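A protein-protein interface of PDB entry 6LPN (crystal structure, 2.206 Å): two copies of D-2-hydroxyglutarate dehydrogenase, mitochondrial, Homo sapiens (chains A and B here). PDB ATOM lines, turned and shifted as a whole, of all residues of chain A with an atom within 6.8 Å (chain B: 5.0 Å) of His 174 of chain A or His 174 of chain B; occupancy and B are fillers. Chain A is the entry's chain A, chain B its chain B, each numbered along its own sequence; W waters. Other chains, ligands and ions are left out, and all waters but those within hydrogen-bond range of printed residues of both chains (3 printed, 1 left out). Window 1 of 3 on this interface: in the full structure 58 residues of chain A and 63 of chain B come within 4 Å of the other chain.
Of the 10 printed residues of chain B, 4 touch a printed residue of chain A.
Of the 18 printed residues of chain A, 4 touch a printed residue of chain B.
Hydrophobic or aromatic side chains of chain A within 4 Å of the printed part of chain B: His 174.
Among the printed residues, 7 pairs touch across the chains.
Among the printed residues, no Asp or Glu carboxylate lies within 4 Å of a Lys or Arg side-chain nitrogen of the other chain.
The side-chain carboxylate (OD1) of Asp 204 of chain A lies within salt-bridge range of the side-chain amino group (NZ) of Lys 206 of chain A (2.9 Å).
OD1 of Asn 161 of chain B is in hydrogen-bond range of OG of Ser 172 of chain B, 3.5 Å away.
A ring nitrogen (ND1) of His 174 of chain A is in hydrogen-bond range of the side-chain amide oxygen (OE1) of Gln 207 of chain A.
N of His 174 of chain B sits at hydrogen-bond distance from OG of Ser 172 of chain B (2.9 Å).
A ring nitrogen (NE2) of His 174 of chain B lies within hydrogen-bond range of the side-chain amide nitrogen (ND2) of Asn 161 of chain B.
ND1 of His 174 of chain B is in hydrogen-bond range of OE1 of Gln 207 of chain B (2.7 Å).
His 174 of chain A touches its own counterpart, His 174 of chain B.
His 174 of chain A touches Asp 204 of chain B, and with the chains exchanged Asp 204 of chain A touches His 174 of chain B.
His 174 of chain A touches Gln 207 of chain B, and with the chains exchanged Gln 207 of chain A touches His 174 of chain B.
Gln 207 of chain A touches its own counterpart, Gln 207 of chain B.
Positions printed for both chains: 161, 172, 173, 174, 175, 176, 177, 204, 207 and 210.
Of the 7 pairs that touch across the chains among the printed residues, 6 have their exchanged pair printed and touching as well.
OD2 of Asp 204 of chain B sits at hydrogen-bond distance from NE2 of His 174 of chain A (3.0 Å).
The side-chain carboxylate (OD2) of Asp 204 of chain A sits at hydrogen-bond distance from a ring nitrogen (NE2) of His 174 of chain B.
The side-chain amide nitrogen of Asn 161 of chain B is in hydrogen-bond range of the side-chain amide oxygen of Asn 200 of chain A, at 2.9 Å.
Asn 161 of chain A touches none of the printed residues of chain B.
Of chain B, only His 174, Asp 204 and Gln 207 come within 4 Å of His 174 of chain A.
Of the printed residues of chain A, Asn 161 of chain B touches Asn 200 (2.9 Å).
Printed residues of chain A within 4 Å of Gln 207 of chain B: His 174 and Gln 207.
The nearest residue of chain B that does not touch His 174 of chain A is Gly 175 of chain B (4.9 Å).
Water W2 lies within hydrogen-bond range of O of Ile 210 of chain B (2.5 Å), N of Asp 204 of chain A (2.9 Å) and O of Gln 207 of chain B (3.5 Å).
Water W3 lies within hydrogen-bond range of the backbone NH (N) of Ser 172 of chain A (2.8 Å) and the backbone carbonyl oxygen (O) of Gly 175 of chain B (3.3 Å).
Water W1 lies within hydrogen-bond range of the backbone NH (N) of Ser 172 of chain B and the backbone carbonyl oxygen (O) of Gly 175 of chain A.
His 174 of chain B touches His 174 of chain A.
CG of His 174 of chain A touches NE2 of Gln 207 of chain B, 3.8 Å away.
Gln 207 of chain A touches His 174 of chain B.
CB of Gln 207 of chain A touches CB of Gln 207 of chain B, 3.6 Å away.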
ATOM      1  N   VAL A 158      17.603  14.289  23.100  1.00  0.00           N
ATOM      2  CA  VAL A 158      17.189  15.332  22.163  1.00  0.00           C
ATOM      3  C   VAL A 158      16.423  16.440  22.883  1.00  0.00           C
ATOM      4  O   VAL A 158      16.644  17.630  22.628  1.00  0.00           O
ATOM      5  CB  VAL A 158      16.368  14.730  21.005  1.00  0.00           C
ATOM      6  CG1 VAL A 158      15.932  15.831  20.051  1.00  0.00           C
ATOM      7  CG2 VAL A 158      17.186  13.694  20.250  1.00  0.00           C
ATOM      8  N   ASN A 161      18.882  18.550  24.658  1.00  0.00           N
ATOM      9  CA  ASN A 161      20.037  18.940  23.846  1.00  0.00           C
ATOM     10  C   ASN A 161      21.337  18.538  24.546  1.00  0.00           C
ATOM     11  O   ASN A 161      22.235  19.349  24.794  1.00  0.00           O
ATOM     12  CB  ASN A 161      20.014  20.446  23.552  1.00  0.00           C
ATOM     13  CG  ASN A 161      21.145  20.887  22.628  1.00  0.00           C
ATOM     14  OD1 ASN A 161      21.524  20.168  21.697  1.00  0.00           O
ATOM     15  ND2 ASN A 161      21.694  22.073  22.890  1.00  0.00           N
ATOM     16  N   GLY A 171      30.002  17.336  17.666  1.00  0.00           N
ATOM     17  CA  GLY A 171      29.195  18.539  17.802  1.00  0.00           C
ATOM     18  C   GLY A 171      27.769  18.274  18.269  1.00  0.00           C
ATOM     19  O   GLY A 171      27.421  17.221  18.817  1.00  0.00           O
ATOM     20  N   SER A 172      26.932  19.275  18.031  1.00  0.00           N
ATOM     21  CA  SER A 172      25.628  19.398  18.665  1.00  0.00           C
ATOM     22  C   SER A 172      24.592  18.493  18.006  1.00  0.00           C
ATOM     23  O   SER A 172      24.698  18.140  16.828  1.00  0.00           O
ATOM     24  CB  SER A 172      25.152  20.854  18.589  1.00  0.00           C
ATOM     25  OG  SER A 172      23.847  20.987  19.124  1.00  0.00           O
ATOM     26  N   LEU A 173      23.595  18.088  18.803  1.00  0.00           N
ATOM     27  CA  LEU A 173      22.398  17.457  18.249  1.00  0.00           C
ATOM     28  C   LEU A 173      21.658  18.370  17.280  1.00  0.00           C
ATOM     29  O   LEU A 173      20.980  17.885  16.368  1.00  0.00           O
ATOM     30  CB  LEU A 173      21.455  17.039  19.376  1.00  0.00           C
ATOM     31  CG  LEU A 173      21.952  15.894  20.249  1.00  0.00           C
ATOM     32  CD1 LEU A 173      21.082  15.791  21.497  1.00  0.00           C
ATOM     33  CD2 LEU A 173      21.917  14.610  19.451  1.00  0.00           C
ATOM     34  N   HIS A 174      21.782  19.688  17.450  1.00  0.00           N
ATOM     35  CA  HIS A 174      21.247  20.619  16.458  1.00  0.00           C
ATOM     36  C   HIS A 174      21.816  20.341  15.075  1.00  0.00           C
ATOM     37  O   HIS A 174      21.161  20.646  14.073  1.00  0.00           O
ATOM     38  CB  HIS A 174      21.494  22.072  16.892  1.00  0.00           C
ATOM     39  CG  HIS A 174      20.670  22.479  18.069  1.00  0.00           C
ATOM     40  ND1 HIS A 174      19.307  22.679  17.993  1.00  0.00           N
ATOM     41  CD2 HIS A 174      21.006  22.680  19.366  1.00  0.00           C
ATOM     42  CE1 HIS A 174      18.845  23.004  19.188  1.00  0.00           C
ATOM     43  NE2 HIS A 174      19.855  23.005  20.040  1.00  0.00           N
ATOM     44  N   GLY A 175      23.029  19.785  15.000  1.00  0.00           N
ATOM     45  CA  GLY A 175      23.620  19.337  13.746  1.00  0.00           C
ATOM     46  C   GLY A 175      23.448  17.869  13.374  1.00  0.00           C
ATOM     47  O   GLY A 175      23.336  17.544  12.190  1.00  0.00           O
ATOM     48  N   THR A 176      23.462  16.961  14.350  1.00  0.00           N
ATOM     49  CA  THR A 176      23.468  15.530  14.049  1.00  0.00           C
ATOM     50  C   THR A 176      22.074  14.922  13.937  1.00  0.00           C
ATOM     51  O   THR A 176      21.927  13.860  13.319  1.00  0.00           O
ATOM     52  CB  THR A 176      24.289  14.758  15.097  1.00  0.00           C
ATOM     53  OG1 THR A 176      23.744  14.970  16.409  1.00  0.00           O
ATOM     54  CG2 THR A 176      25.749  15.190  15.066  1.00  0.00           C
ATOM     55  N   VAL A 177      21.060  15.558  14.514  1.00  0.00           N
ATOM     56  CA  VAL A 177      19.680  15.105  14.378  1.00  0.00           C
ATOM     57  C   VAL A 177      19.157  15.502  13.004  1.00  0.00           C
ATOM     58  O   VAL A 177      19.207  16.677  12.627  1.00  0.00           O
ATOM     59  CB  VAL A 177      18.804  15.689  15.496  1.00  0.00           C
ATOM     60  CG1 VAL A 177      17.327  15.414  15.227  1.00  0.00           C
ATOM     61  CG2 VAL A 177      19.209  15.103  16.834  1.00  0.00           C
ATOM     62  N   ASN A 200      16.564  22.262   2.506  1.00  0.00           N
ATOM     63  CA  ASN A 200      16.174  23.650   2.774  1.00  0.00           C
ATOM     64  C   ASN A 200      14.805  24.000   2.191  1.00  0.00           C
ATOM     65  O   ASN A 200      14.651  24.998   1.473  1.00  0.00           O
ATOM     66  CB  ASN A 200      17.250  24.608   2.277  1.00  0.00           C
ATOM     67  CG  ASN A 200      18.419  24.701   3.228  1.00  0.00           C
ATOM     68  OD1 ASN A 200      18.381  24.139   4.321  1.00  0.00           O
ATOM     69  ND2 ASN A 200      19.468  25.396   2.817  1.00  0.00           N
ATOM     70  N   TYR A 203      11.168  26.292   7.010  1.00  0.00           N
ATOM     71  CA  TYR A 203      11.757  26.482   8.323  1.00  0.00           C
ATOM     72  C   TYR A 203      12.157  25.140   8.919  1.00  0.00           C
ATOM     73  O   TYR A 203      11.487  24.124   8.715  1.00  0.00           O
ATOM     74  CB  TYR A 203      10.774  27.179   9.269  1.00  0.00           C
ATOM     75  CG  TYR A 203      10.177  28.488   8.790  1.00  0.00           C
ATOM     76  CD1 TYR A 203      10.845  29.310   7.882  1.00  0.00           C
ATOM     77  CD2 TYR A 203       8.952  28.919   9.284  1.00  0.00           C
ATOM     78  CE1 TYR A 203      10.292  30.518   7.469  1.00  0.00           C
ATOM     79  CE2 TYR A 203       8.392  30.132   8.880  1.00  0.00           C
ATOM     80  CZ  TYR A 203       9.061  30.924   7.975  1.00  0.00           C
ATOM     81  OH  TYR A 203       8.490  32.118   7.586  1.00  0.00           O
ATOM     82  N   ASP A 204      13.276  25.139   9.645  1.00  0.00           N
ATOM     83  CA  ASP A 204      13.805  23.932  10.280  1.00  0.00           C
ATOM     84  C   ASP A 204      13.110  23.709  11.626  1.00  0.00           C
ATOM     85  O   ASP A 204      13.690  23.854  12.703  1.00  0.00           O
ATOM     86  CB  ASP A 204      15.313  24.026  10.446  1.00  0.00           C
ATOM     87  CG  ASP A 204      15.953  22.673  10.672  1.00  0.00           C
ATOM     88  OD1 ASP A 204      15.210  21.670  10.795  1.00  0.00           O
ATOM     89  OD2 ASP A 204      17.195  22.616  10.772  1.00  0.00           O
ATOM     90  N   LYS A 206      12.157  21.173  13.403  1.00  0.00           N
ATOM     91  CA  LYS A 206      12.627  20.215  14.407  1.00  0.00           C
ATOM     92  C   LYS A 206      13.541  20.865  15.445  1.00  0.00           C
ATOM     93  O   LYS A 206      13.561  20.433  16.601  1.00  0.00           O
ATOM     94  CB  LYS A 206      13.343  19.038  13.742  1.00  0.00           C
ATOM     95  CG  LYS A 206      14.723  19.364  13.212  1.00  0.00           C
ATOM     96  CD  LYS A 206      15.360  18.176  12.520  1.00  0.00           C
ATOM     97  CE  LYS A 206      16.777  18.513  12.083  1.00  0.00           C
ATOM     98  NZ  LYS A 206      16.805  19.258  10.810  1.00  0.00           N
ATOM     99  N   GLN A 207      14.310  21.884  15.036  1.00  0.00           N
ATOM    100  CA  GLN A 207      15.253  22.583  15.912  1.00  0.00           C
ATOM    101  C   GLN A 207      14.601  23.164  17.165  1.00  0.00           C
ATOM    102  O   GLN A 207      15.240  23.225  18.223  1.00  0.00           O
ATOM    103  CB  GLN A 207      15.940  23.704  15.125  1.00  0.00           C
ATOM    104  CG  GLN A 207      16.815  23.246  13.976  1.00  0.00           C
ATOM    105  CD  GLN A 207      18.068  22.529  14.470  1.00  0.00           C
ATOM    106  OE1 GLN A 207      18.333  22.483  15.669  1.00  0.00           O
ATOM    107  NE2 GLN A 207      18.836  21.971  13.552  1.00  0.00           N
ATOM    108  N   LEU A 208      13.351  23.618  17.059  1.00  0.00           N
ATOM    109  CA  LEU A 208      12.623  24.121  18.222  1.00  0.00           C
ATOM    110  C   LEU A 208      12.482  23.097  19.330  1.00  0.00           C
ATOM    111  O   LEU A 208      12.478  23.467  20.512  1.00  0.00           O
ATOM    112  CB  LEU A 208      11.228  24.579  17.807  1.00  0.00           C
ATOM    113  CG  LEU A 208      11.129  25.861  17.000  1.00  0.00           C
ATOM    114  CD1 LEU A 208       9.675  26.122  16.654  1.00  0.00           C
ATOM    115  CD2 LEU A 208      11.686  26.984  17.842  1.00  0.00           C
ATOM    116  N   PHE A 209      12.410  21.813  18.986  1.00  0.00           N
ATOM    117  CA  PHE A 209      12.154  20.775  19.971  1.00  0.00           C
ATOM    118  C   PHE A 209      13.425  20.170  20.548  1.00  0.00           C
ATOM    119  O   PHE A 209      13.350  19.434  21.537  1.00  0.00           O
ATOM    120  CB  PHE A 209      11.279  19.684  19.341  1.00  0.00           C
ATOM    121  CG  PHE A 209       9.967  20.204  18.824  1.00  0.00           C
ATOM    122  CD1 PHE A 209       8.879  20.348  19.672  1.00  0.00           C
ATOM    123  CD2 PHE A 209       9.833  20.590  17.506  1.00  0.00           C
ATOM    124  CE1 PHE A 209       7.684  20.842  19.205  1.00  0.00           C
ATOM    125  CE2 PHE A 209       8.637  21.090  17.035  1.00  0.00           C
ATOM    126  CZ  PHE A 209       7.562  21.213  17.882  1.00  0.00           C
ATOM    127  N   ILE A 210      14.580  20.511  19.995  1.00  0.00           N
ATOM    128  CA  ILE A 210      15.859  20.044  20.507  1.00  0.00           C
ATOM    129  C   ILE A 210      16.263  21.045  21.581  1.00  0.00           C
ATOM    130  O   ILE A 210      16.601  22.194  21.277  1.00  0.00           O
ATOM    131  CB  ILE A 210      16.906  19.945  19.388  1.00  0.00           C
ATOM    132  CG1 ILE A 210      16.408  19.021  18.267  1.00  0.00           C
ATOM    133  CG2 ILE A 210      18.266  19.501  19.926  1.00  0.00           C
ATOM    134  CD1 ILE A 210      17.273  19.046  17.027  1.00  0.00           C
ATOM    135  N   GLY A 211      16.293  20.591  22.833  1.00  0.00           N
ATOM    136  CA  GLY A 211      16.491  21.484  23.953  1.00  0.00           C
ATOM    137  C   GLY A 211      15.224  22.087  24.537  1.00  0.00           C
ATOM    138  O   GLY A 211      15.320  22.935  25.426  1.00  0.00           O
ATOM    139  N   ASN B 161      20.578  29.222   5.092  1.00  0.00           N
ATOM    140  CA  ASN B 161      21.217  28.011   5.622  1.00  0.00           C
ATOM    141  C   ASN B 161      22.119  27.355   4.567  1.00  0.00           C
ATOM    142  O   ASN B 161      21.985  26.173   4.237  1.00  0.00           O
ATOM    143  CB  ASN B 161      20.164  27.022   6.136  1.00  0.00           C
ATOM    144  CG  ASN B 161      20.786  25.778   6.760  1.00  0.00           C
ATOM    145  OD1 ASN B 161      21.839  25.849   7.406  1.00  0.00           O
ATOM    146  ND2 ASN B 161      20.170  24.628   6.521  1.00  0.00           N
ATOM    147  N   SER B 172      26.462  21.699   9.186  1.00  0.00           N
ATOM    148  CA  SER B 172      25.474  22.751   8.982  1.00  0.00           C
ATOM    149  C   SER B 172      25.769  24.013   9.793  1.00  0.00           C
ATOM    150  O   SER B 172      26.379  23.973  10.865  1.00  0.00           O
ATOM    151  CB  SER B 172      24.084  22.219   9.354  1.00  0.00           C
ATOM    152  OG  SER B 172      23.095  23.231   9.274  1.00  0.00           O
ATOM    153  N   LEU B 173      25.274  25.142   9.274  1.00  0.00           N
ATOM    154  CA  LEU B 173      25.215  26.384  10.040  1.00  0.00           C
ATOM    155  C   LEU B 173      24.368  26.229  11.302  1.00  0.00           C
ATOM    156  O   LEU B 173      24.617  26.907  12.309  1.00  0.00           O
ATOM    157  CB  LEU B 173      24.668  27.499   9.143  1.00  0.00           C
ATOM    158  CG  LEU B 173      25.608  27.950   8.018  1.00  0.00           C
ATOM    159  CD1 LEU B 173      24.915  28.907   7.056  1.00  0.00           C
ATOM    160  CD2 LEU B 173      26.845  28.620   8.635  1.00  0.00           C
ATOM    161  N   HIS B 174      23.391  25.322  11.276  1.00  0.00           N
ATOM    162  CA  HIS B 174      22.642  24.980  12.482  1.00  0.00           C
ATOM    163  C   HIS B 174      23.553  24.495  13.603  1.00  0.00           C
ATOM    164  O   HIS B 174      23.199  24.626  14.781  1.00  0.00           O
ATOM    165  CB  HIS B 174      21.577  23.920  12.165  1.00  0.00           C
ATOM    166  CG  HIS B 174      20.441  24.425  11.324  1.00  0.00           C
ATOM    167  ND1 HIS B 174      19.448  25.237  11.828  1.00  0.00           N
ATOM    168  CD2 HIS B 174      20.134  24.225  10.020  1.00  0.00           C
ATOM    169  CE1 HIS B 174      18.579  25.518  10.871  1.00  0.00           C
ATOM    170  NE2 HIS B 174      18.977  24.922   9.762  1.00  0.00           N
ATOM    171  N   GLY B 175      24.721  23.941  13.262  1.00  0.00           N
ATOM    172  CA  GLY B 175      25.743  23.597  14.240  1.00  0.00           C
ATOM    173  C   GLY B 175      26.819  24.635  14.505  1.00  0.00           C
ATOM    174  O   GLY B 175      27.318  24.726  15.627  1.00  0.00           O
ATOM    175  N   THR B 176      27.248  25.366  13.480  1.00  0.00           N
ATOM    176  CA  THR B 176      28.396  26.261  13.590  1.00  0.00           C
ATOM    177  C   THR B 176      28.033  27.691  13.991  1.00  0.00           C
ATOM    178  O   THR B 176      28.914  28.434  14.429  1.00  0.00           O
ATOM    179  CB  THR B 176      29.168  26.287  12.271  1.00  0.00           C
ATOM    180  OG1 THR B 176      28.259  26.592  11.210  1.00  0.00           O
ATOM    181  CG2 THR B 176      29.801  24.920  12.012  1.00  0.00           C
ATOM    182  N   VAL B 177      26.787  28.119  13.792  1.00  0.00           N
ATOM    183  CA  VAL B 177      26.358  29.422  14.289  1.00  0.00           C
ATOM    184  C   VAL B 177      26.179  29.333  15.804  1.00  0.00           C
ATOM    185  O   VAL B 177      25.397  28.522  16.313  1.00  0.00           O
ATOM    186  CB  VAL B 177      25.070  29.882  13.584  1.00  0.00           C
ATOM    187  CG1 VAL B 177      24.530  31.152  14.227  1.00  0.00           C
ATOM    188  CG2 VAL B 177      25.332  30.125  12.086  1.00  0.00           C
ATOM    189  N   ASP B 204      16.386  27.303  21.766  1.00  0.00           N
ATOM    190  CA  ASP B 204      17.433  27.734  20.841  1.00  0.00           C
ATOM    191  C   ASP B 204      16.778  28.629  19.781  1.00  0.00           C
ATOM    192  O   ASP B 204      16.530  28.231  18.644  1.00  0.00           O
ATOM    193  CB  ASP B 204      18.111  26.509  20.234  1.00  0.00           C
ATOM    194  CG  ASP B 204      19.497  26.801  19.676  1.00  0.00           C
ATOM    195  OD1 ASP B 204      19.975  27.951  19.766  1.00  0.00           O
ATOM    196  OD2 ASP B 204      20.108  25.853  19.134  1.00  0.00           O
ATOM    197  N   GLN B 207      17.866  29.281  16.053  1.00  0.00           N
ATOM    198  CA  GLN B 207      17.635  28.261  15.034  1.00  0.00           C
ATOM    199  C   GLN B 207      16.483  28.627  14.101  1.00  0.00           C
ATOM    200  O   GLN B 207      16.503  28.261  12.922  1.00  0.00           O
ATOM    201  CB  GLN B 207      17.337  26.921  15.695  1.00  0.00           C
ATOM    202  CG  GLN B 207      18.474  26.348  16.491  1.00  0.00           C
ATOM    203  CD  GLN B 207      19.721  26.066  15.670  1.00  0.00           C
ATOM    204  OE1 GLN B 207      19.671  25.946  14.445  1.00  0.00           O
ATOM    205  NE2 GLN B 207      20.848  25.920  16.358  1.00  0.00           N
ATOM    206  N   ILE B 210      17.793  30.572  11.098  1.00  0.00           N
ATOM    207  CA  ILE B 210      18.688  29.877  10.180  1.00  0.00           C
ATOM    208  C   ILE B 210      17.818  29.145   9.165  1.00  0.00           C
ATOM    209  O   ILE B 210      17.073  28.227   9.515  1.00  0.00           O
ATOM    210  CB  ILE B 210      19.611  28.911  10.937  1.00  0.00           C
ATOM    211  CG1 ILE B 210      20.413  29.694  11.987  1.00  0.00           C
ATOM    212  CG2 ILE B 210      20.549  28.159   9.973  1.00  0.00           C
ATOM    213  CD1 ILE B 210      21.336  28.845  12.842  1.00  0.00           C
HETATM  214  O   HOH W   1      25.605  19.191  10.482  1.00  0.00           O
HETATM  215  O   HOH W   2      14.644  27.664  10.018  1.00  0.00           O
HETATM  216  O   HOH W   3      27.709  21.661  16.852  1.00  0.00           O
